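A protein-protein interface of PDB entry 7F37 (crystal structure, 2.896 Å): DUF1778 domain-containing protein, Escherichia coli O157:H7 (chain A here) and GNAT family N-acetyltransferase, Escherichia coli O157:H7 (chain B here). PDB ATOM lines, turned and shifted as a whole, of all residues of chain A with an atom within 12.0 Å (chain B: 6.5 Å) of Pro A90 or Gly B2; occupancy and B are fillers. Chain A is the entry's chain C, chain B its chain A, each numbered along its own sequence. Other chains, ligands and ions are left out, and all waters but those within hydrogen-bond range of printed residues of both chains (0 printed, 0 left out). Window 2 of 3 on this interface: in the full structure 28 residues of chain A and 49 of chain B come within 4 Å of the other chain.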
ATOM      1  N   ALA A  83     -25.250 -10.018 -15.725  1.00  0.00           N
ATOM      2  CA  ALA A  83     -24.378 -10.932 -14.988  1.00  0.00           C
ATOM      3  C   ALA A  83     -23.065 -11.156 -15.714  1.00  0.00           C
ATOM      4  O   ALA A  83     -22.007 -11.255 -15.080  1.00  0.00           O
ATOM      5  CB  ALA A  83     -25.069 -12.271 -14.772  1.00  0.00           C
ATOM      6  N   LEU A  84     -23.117 -11.272 -17.046  1.00  0.00           N
ATOM      7  CA  LEU A  84     -21.912 -11.529 -17.825  1.00  0.00           C
ATOM      8  C   LEU A  84     -20.952 -10.351 -17.739  1.00  0.00           C
ATOM      9  O   LEU A  84     -19.790 -10.506 -17.347  1.00  0.00           O
ATOM     10  CB  LEU A  84     -22.294 -11.832 -19.277  1.00  0.00           C
ATOM     11  CG  LEU A  84     -21.140 -12.085 -20.244  1.00  0.00           C
ATOM     12  CD1 LEU A  84     -20.429 -13.391 -19.913  1.00  0.00           C
ATOM     13  CD2 LEU A  84     -21.625 -12.068 -21.685  1.00  0.00           C
ATOM     14  N   MET A  85     -21.443  -9.154 -18.048  1.00  0.00           N
ATOM     15  CA  MET A  85     -20.615  -7.964 -18.148  1.00  0.00           C
ATOM     16  C   MET A  85     -20.223  -7.350 -16.808  1.00  0.00           C
ATOM     17  O   MET A  85     -19.347  -6.481 -16.801  1.00  0.00           O
ATOM     18  CB  MET A  85     -21.341  -6.913 -18.976  1.00  0.00           C
ATOM     19  CG  MET A  85     -22.032  -7.481 -20.182  1.00  0.00           C
ATOM     20  SD  MET A  85     -20.989  -7.582 -21.640  1.00  0.00           S
ATOM     21  CE  MET A  85     -21.742  -6.286 -22.630  1.00  0.00           C
ATOM     22  N   ASN A  86     -20.846  -7.741 -15.689  1.00  0.00           N
ATOM     23  CA  ASN A  86     -20.416  -7.218 -14.388  1.00  0.00           C
ATOM     24  C   ASN A  86     -19.247  -7.999 -13.799  1.00  0.00           C
ATOM     25  O   ASN A  86     -18.420  -7.422 -13.078  1.00  0.00           O
ATOM     26  CB  ASN A  86     -21.557  -7.250 -13.377  1.00  0.00           C
ATOM     27  CG  ASN A  86     -22.607  -6.206 -13.634  1.00  0.00           C
ATOM     28  OD1 ASN A  86     -22.573  -5.501 -14.628  1.00  0.00           O
ATOM     29  ND2 ASN A  86     -23.566  -6.115 -12.733  1.00  0.00           N
ATOM     30  N   ARG A  87     -19.203  -9.308 -14.051  1.00  0.00           N
ATOM     31  CA  ARG A  87     -18.141 -10.174 -13.554  1.00  0.00           C
ATOM     32  C   ARG A  87     -16.808  -9.677 -14.065  1.00  0.00           C
ATOM     33  O   ARG A  87     -16.621  -9.543 -15.281  1.00  0.00           O
ATOM     34  CB  ARG A  87     -18.391 -11.604 -14.021  1.00  0.00           C
ATOM     35  CG  ARG A  87     -19.577 -12.285 -13.370  1.00  0.00           C
ATOM     36  CD  ARG A  87     -19.190 -13.688 -12.991  1.00  0.00           C
ATOM     37  NE  ARG A  87     -17.931 -13.645 -12.269  1.00  0.00           N
ATOM     38  CZ  ARG A  87     -17.393 -14.666 -11.614  1.00  0.00           C
ATOM     39  NH1 ARG A  87     -18.007 -15.859 -11.564  1.00  0.00           N
ATOM     40  NH2 ARG A  87     -16.231 -14.470 -10.999  1.00  0.00           N
ATOM     41  N   LYS A  88     -15.906  -9.349 -13.144  1.00  0.00           N
ATOM     42  CA  LYS A  88     -14.607  -8.820 -13.528  1.00  0.00           C
ATOM     43  C   LYS A  88     -13.624  -9.974 -13.701  1.00  0.00           C
ATOM     44  O   LYS A  88     -13.371 -10.735 -12.754  1.00  0.00           O
ATOM     45  CB  LYS A  88     -14.080  -7.827 -12.504  1.00  0.00           C
ATOM     46  CG  LYS A  88     -12.685  -7.402 -12.828  1.00  0.00           C
ATOM     47  CD  LYS A  88     -12.085  -6.725 -11.618  1.00  0.00           C
ATOM     48  CE  LYS A  88     -10.966  -7.528 -10.985  1.00  0.00           C
ATOM     49  NZ  LYS A  88     -11.552  -8.557 -10.082  1.00  0.00           N
ATOM     50  N   SER A  89     -13.102 -10.115 -14.918  1.00  0.00           N
ATOM     51  CA  SER A  89     -12.215 -11.219 -15.259  1.00  0.00           C
ATOM     52  C   SER A  89     -10.917 -11.115 -14.456  1.00  0.00           C
ATOM     53  O   SER A  89     -10.478 -10.000 -14.151  1.00  0.00           O
ATOM     54  CB  SER A  89     -11.921 -11.179 -16.760  1.00  0.00           C
ATOM     55  OG  SER A  89     -13.050 -10.736 -17.511  1.00  0.00           O
ATOM     56  N   PRO A  90     -10.283 -12.235 -14.079  1.00  0.00           N
ATOM     57  CA  PRO A  90      -9.081 -12.132 -13.244  1.00  0.00           C
ATOM     58  C   PRO A  90      -7.902 -11.478 -13.937  1.00  0.00           C
ATOM     59  O   PRO A  90      -6.849 -11.317 -13.308  1.00  0.00           O
ATOM     60  CB  PRO A  90      -8.774 -13.595 -12.878  1.00  0.00           C
ATOM     61  CG  PRO A  90      -9.398 -14.393 -13.917  1.00  0.00           C
ATOM     62  CD  PRO A  90     -10.596 -13.638 -14.403  1.00  0.00           C
ATOM     63  N   TRP A  91      -8.048 -11.080 -15.196  1.00  0.00           N
ATOM     64  CA  TRP A  91      -7.013 -10.374 -15.947  1.00  0.00           C
ATOM     65  C   TRP A  91      -7.421  -8.933 -16.218  1.00  0.00           C
ATOM     66  O   TRP A  91      -7.075  -8.343 -17.241  1.00  0.00           O
ATOM     67  CB  TRP A  91      -6.715 -11.082 -17.263  1.00  0.00           C
ATOM     68  CG  TRP A  91      -7.887 -11.192 -18.192  1.00  0.00           C
ATOM     69  CD1 TRP A  91      -8.443 -10.198 -18.963  1.00  0.00           C
ATOM     70  CD2 TRP A  91      -8.629 -12.372 -18.464  1.00  0.00           C
ATOM     71  NE1 TRP A  91      -9.490 -10.696 -19.695  1.00  0.00           N
ATOM     72  CE2 TRP A  91      -9.625 -12.032 -19.408  1.00  0.00           C
ATOM     73  CE3 TRP A  91      -8.555 -13.690 -17.996  1.00  0.00           C
ATOM     74  CZ2 TRP A  91     -10.545 -12.961 -19.883  1.00  0.00           C
ATOM     75  CZ3 TRP A  91      -9.454 -14.612 -18.472  1.00  0.00           C
ATOM     76  CH2 TRP A  91     -10.439 -14.246 -19.411  1.00  0.00           C
ATOM     77  N   GLU A  92      -8.151  -8.350 -15.287  1.00  0.00           N
ATOM     78  CA  GLU A  92      -8.905  -7.155 -15.577  1.00  0.00           C
ATOM     79  C   GLU A  92      -8.869  -6.266 -14.343  1.00  0.00           C
ATOM     80  O   GLU A  92      -9.006  -5.050 -14.460  1.00  0.00           O
ATOM     81  CB  GLU A  92     -10.340  -7.539 -15.954  1.00  0.00           C
ATOM     82  CG  GLU A  92     -10.962  -6.806 -17.128  1.00  0.00           C
ATOM     83  CD  GLU A  92     -12.269  -7.467 -17.566  1.00  0.00           C
ATOM     84  OE1 GLU A  92     -12.510  -7.569 -18.795  1.00  0.00           O
ATOM     85  OE2 GLU A  92     -13.044  -7.895 -16.681  1.00  0.00           O
ATOM     86  OXT GLU A  92      -8.693  -6.740 -13.208  1.00  0.00           O
ATOM     87  N   GLY B   2      -3.688 -12.406 -11.381  1.00  0.00           N
ATOM     88  CA  GLY B   2      -2.774 -13.424 -11.888  1.00  0.00           C
ATOM     89  C   GLY B   2      -2.632 -13.605 -13.411  1.00  0.00           C
ATOM     90  O   GLY B   2      -1.551 -13.381 -13.973  1.00  0.00           O
ATOM     91  N   ILE B   3      -3.732 -14.018 -14.074  1.00  0.00           N
ATOM     92  CA  ILE B   3      -3.742 -14.318 -15.511  1.00  0.00           C
ATOM     93  C   ILE B   3      -3.765 -13.025 -16.327  1.00  0.00           C
ATOM     94  O   ILE B   3      -4.146 -11.959 -15.839  1.00  0.00           O
ATOM     95  CB  ILE B   3      -4.950 -15.218 -15.839  1.00  0.00           C
ATOM     96  CG1 ILE B   3      -4.934 -16.442 -14.929  1.00  0.00           C
ATOM     97  CG2 ILE B   3      -4.982 -15.637 -17.301  1.00  0.00           C
ATOM     98  CD1 ILE B   3      -5.899 -17.541 -15.343  1.00  0.00           C
ATOM     99  N   THR B   4      -3.330 -13.112 -17.587  1.00  0.00           N
ATOM    100  CA  THR B   4      -3.410 -11.974 -18.491  1.00  0.00           C
ATOM    101  C   THR B   4      -4.308 -12.283 -19.684  1.00  0.00           C
ATOM    102  O   THR B   4      -4.583 -13.445 -20.009  1.00  0.00           O
ATOM    103  CB  THR B   4      -2.028 -11.529 -18.999  1.00  0.00           C
ATOM    104  OG1 THR B   4      -2.162 -10.297 -19.728  1.00  0.00           O
ATOM    105  CG2 THR B   4      -1.424 -12.580 -19.924  1.00  0.00           C
ATOM    106  N   CYS B  48      -3.162 -17.521 -19.932  1.00  0.00           N
ATOM    107  CA  CYS B  48      -2.000 -18.196 -19.367  1.00  0.00           C
ATOM    108  C   CYS B  48      -1.801 -17.840 -17.900  1.00  0.00           C
ATOM    109  O   CYS B  48      -2.277 -16.809 -17.427  1.00  0.00           O
ATOM    110  CB  CYS B  48      -0.740 -17.834 -20.147  1.00  0.00           C
ATOM    111  SG  CYS B  48      -0.637 -18.634 -21.766  1.00  0.00           S
ATOM    112  N   ILE B  49      -1.033 -18.692 -17.199  1.00  0.00           N
ATOM    113  CA  ILE B  49      -0.681 -18.517 -15.787  1.00  0.00           C
ATOM    114  C   ILE B  49       0.116 -17.226 -15.705  1.00  0.00           C
ATOM    115  O   ILE B  49       0.465 -16.654 -16.743  1.00  0.00           O
ATOM    116  CB  ILE B  49       0.122 -19.705 -15.211  1.00  0.00           C
ATOM    117  CG1 ILE B  49      -0.424 -21.056 -15.686  1.00  0.00           C
ATOM    118  CG2 ILE B  49       0.064 -19.696 -13.699  1.00  0.00           C
ATOM    119  CD1 ILE B  49       0.013 -22.247 -14.859  1.00  0.00           C
ATOM    120  N   ALA B  50       0.423 -16.765 -14.490  1.00  0.00           N
ATOM    121  CA  ALA B  50       0.853 -15.389 -14.241  1.00  0.00           C
ATOM    122  C   ALA B  50       1.702 -14.773 -15.357  1.00  0.00           C
ATOM    123  O   ALA B  50       1.282 -13.791 -15.978  1.00  0.00           O
ATOM    124  CB  ALA B  50       1.637 -15.344 -12.927  1.00  0.00           C
ATOM    125  N   ASN B  51       2.871 -15.358 -15.647  1.00  0.00           N
ATOM    126  CA  ASN B  51       3.656 -15.029 -16.842  1.00  0.00           C
ATOM    127  C   ASN B  51       4.141 -16.269 -17.572  1.00  0.00           C
ATOM    128  O   ASN B  51       4.706 -16.151 -18.664  1.00  0.00           O
ATOM    129  CB  ASN B  51       4.867 -14.147 -16.496  1.00  0.00           C
ATOM    130  CG  ASN B  51       4.470 -12.800 -15.921  1.00  0.00           C
ATOM    131  OD1 ASN B  51       3.762 -12.009 -16.559  1.00  0.00           O
ATOM    132  ND2 ASN B  51       4.920 -12.533 -14.701  1.00  0.00           N
ATOM    133  N   LYS B 100     -12.939 -21.530 -10.555  1.00  0.00           N
ATOM    134  CA  LYS B 100     -12.263 -20.271 -10.356  1.00  0.00           C
ATOM    135  C   LYS B 100     -12.837 -19.171 -11.264  1.00  0.00           C
ATOM    136  O   LYS B 100     -12.174 -18.151 -11.522  1.00  0.00           O
ATOM    137  CB  LYS B 100     -10.756 -20.487 -10.530  1.00  0.00           C
ATOM    138  CG  LYS B 100     -10.305 -21.822  -9.883  1.00  0.00           C
ATOM    139  CD  LYS B 100      -8.864 -21.827  -9.355  1.00  0.00           C
ATOM    140  CE  LYS B 100      -8.439 -23.220  -8.818  1.00  0.00           C
ATOM    141  NZ  LYS B 100      -9.109 -23.611  -7.542  1.00  0.00           N
ATOM    142  N   GLY B 101     -14.067 -19.390 -11.743  1.00  0.00           N
ATOM    143  CA  GLY B 101     -14.826 -18.393 -12.476  1.00  0.00           C
ATOM    144  C   GLY B 101     -14.273 -18.041 -13.838  1.00  0.00           C
ATOM    145  O   GLY B 101     -14.545 -16.944 -14.350  1.00  0.00           O
ATOM    146  N   LEU B 102     -13.522 -18.956 -14.459  1.00  0.00           N
ATOM    147  CA  LEU B 102     -12.737 -18.626 -15.643  1.00  0.00           C
ATOM    148  C   LEU B 102     -13.525 -18.746 -16.948  1.00  0.00           C
ATOM    149  O   LEU B 102     -13.273 -17.965 -17.878  1.00  0.00           O
ATOM    150  CB  LEU B 102     -11.483 -19.507 -15.694  1.00  0.00           C
ATOM    151  CG  LEU B 102     -10.245 -18.906 -15.008  1.00  0.00           C
ATOM    152  CD1 LEU B 102      -8.997 -19.739 -15.256  1.00  0.00           C
ATOM    153  CD2 LEU B 102     -10.019 -17.457 -15.425  1.00  0.00           C
ATOM    154  N   ALA B 105     -15.314 -15.658 -17.978  1.00  0.00           N
ATOM    155  CA  ALA B 105     -14.355 -14.614 -18.318  1.00  0.00           C
ATOM    156  C   ALA B 105     -13.962 -14.678 -19.796  1.00  0.00           C
ATOM    157  O   ALA B 105     -13.816 -13.640 -20.466  1.00  0.00           O
ATOM    158  CB  ALA B 105     -13.145 -14.749 -17.406  1.00  0.00           C
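The backbone NH (N) of Ser A89 lies within hydrogen-bond range of the side-chain carboxylate (OE2) of Glu A92, 2.8 Å away.
Among the printed residues, merely in contact across the chains: Trp A91 with Ile B3 (3.1 Å), Trp A91 with Ala B105 (3.4 Å), Pro A90 with Leu B102 (3.5 Å), Trp A91 with Thr B4 (3.6 Å), Pro A90 with Ile B3 (3.8 Å), Ser A89 with Ala B105 (3.8 Å) and Pro A90 with Gly B2 (3.9 Å).
Leu A84 touches none of the printed residues of chain B.
Printed residues of chain B within 4 Å of Ser A89: Ala B105.
Pro A90 touches just these residues of chain B: Gly B2 (3.9 Å), Ile B3 (3.8 Å) and Leu B102 (3.5 Å).
Of the printed residues of chain B, Trp A91 touches Ile B3 (3.1 Å), Thr B4 (3.6 Å) and Ala B105 (3.4 Å).
Of chain A, only Pro A90 and Trp A91 come within 4 Å of Ile B3.
Thr B4 touches just one residue of chain A: Trp A91 (3.6 Å).
No residue of chain A comes within 4 Å of Gly B101.
Of the printed residues of chain A, Leu B102 touches Pro A90 (3.5 Å).
The nearest residue of chain A that does not touch Gly B2 is Trp A91 (5.9 Å).
Of the 10 printed residues of chain A, 3 touch a printed residue of chain B.
Hydrophobic or aromatic side chains of chain B that line the printed part of chain A: Leu B102 and Ala B105.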
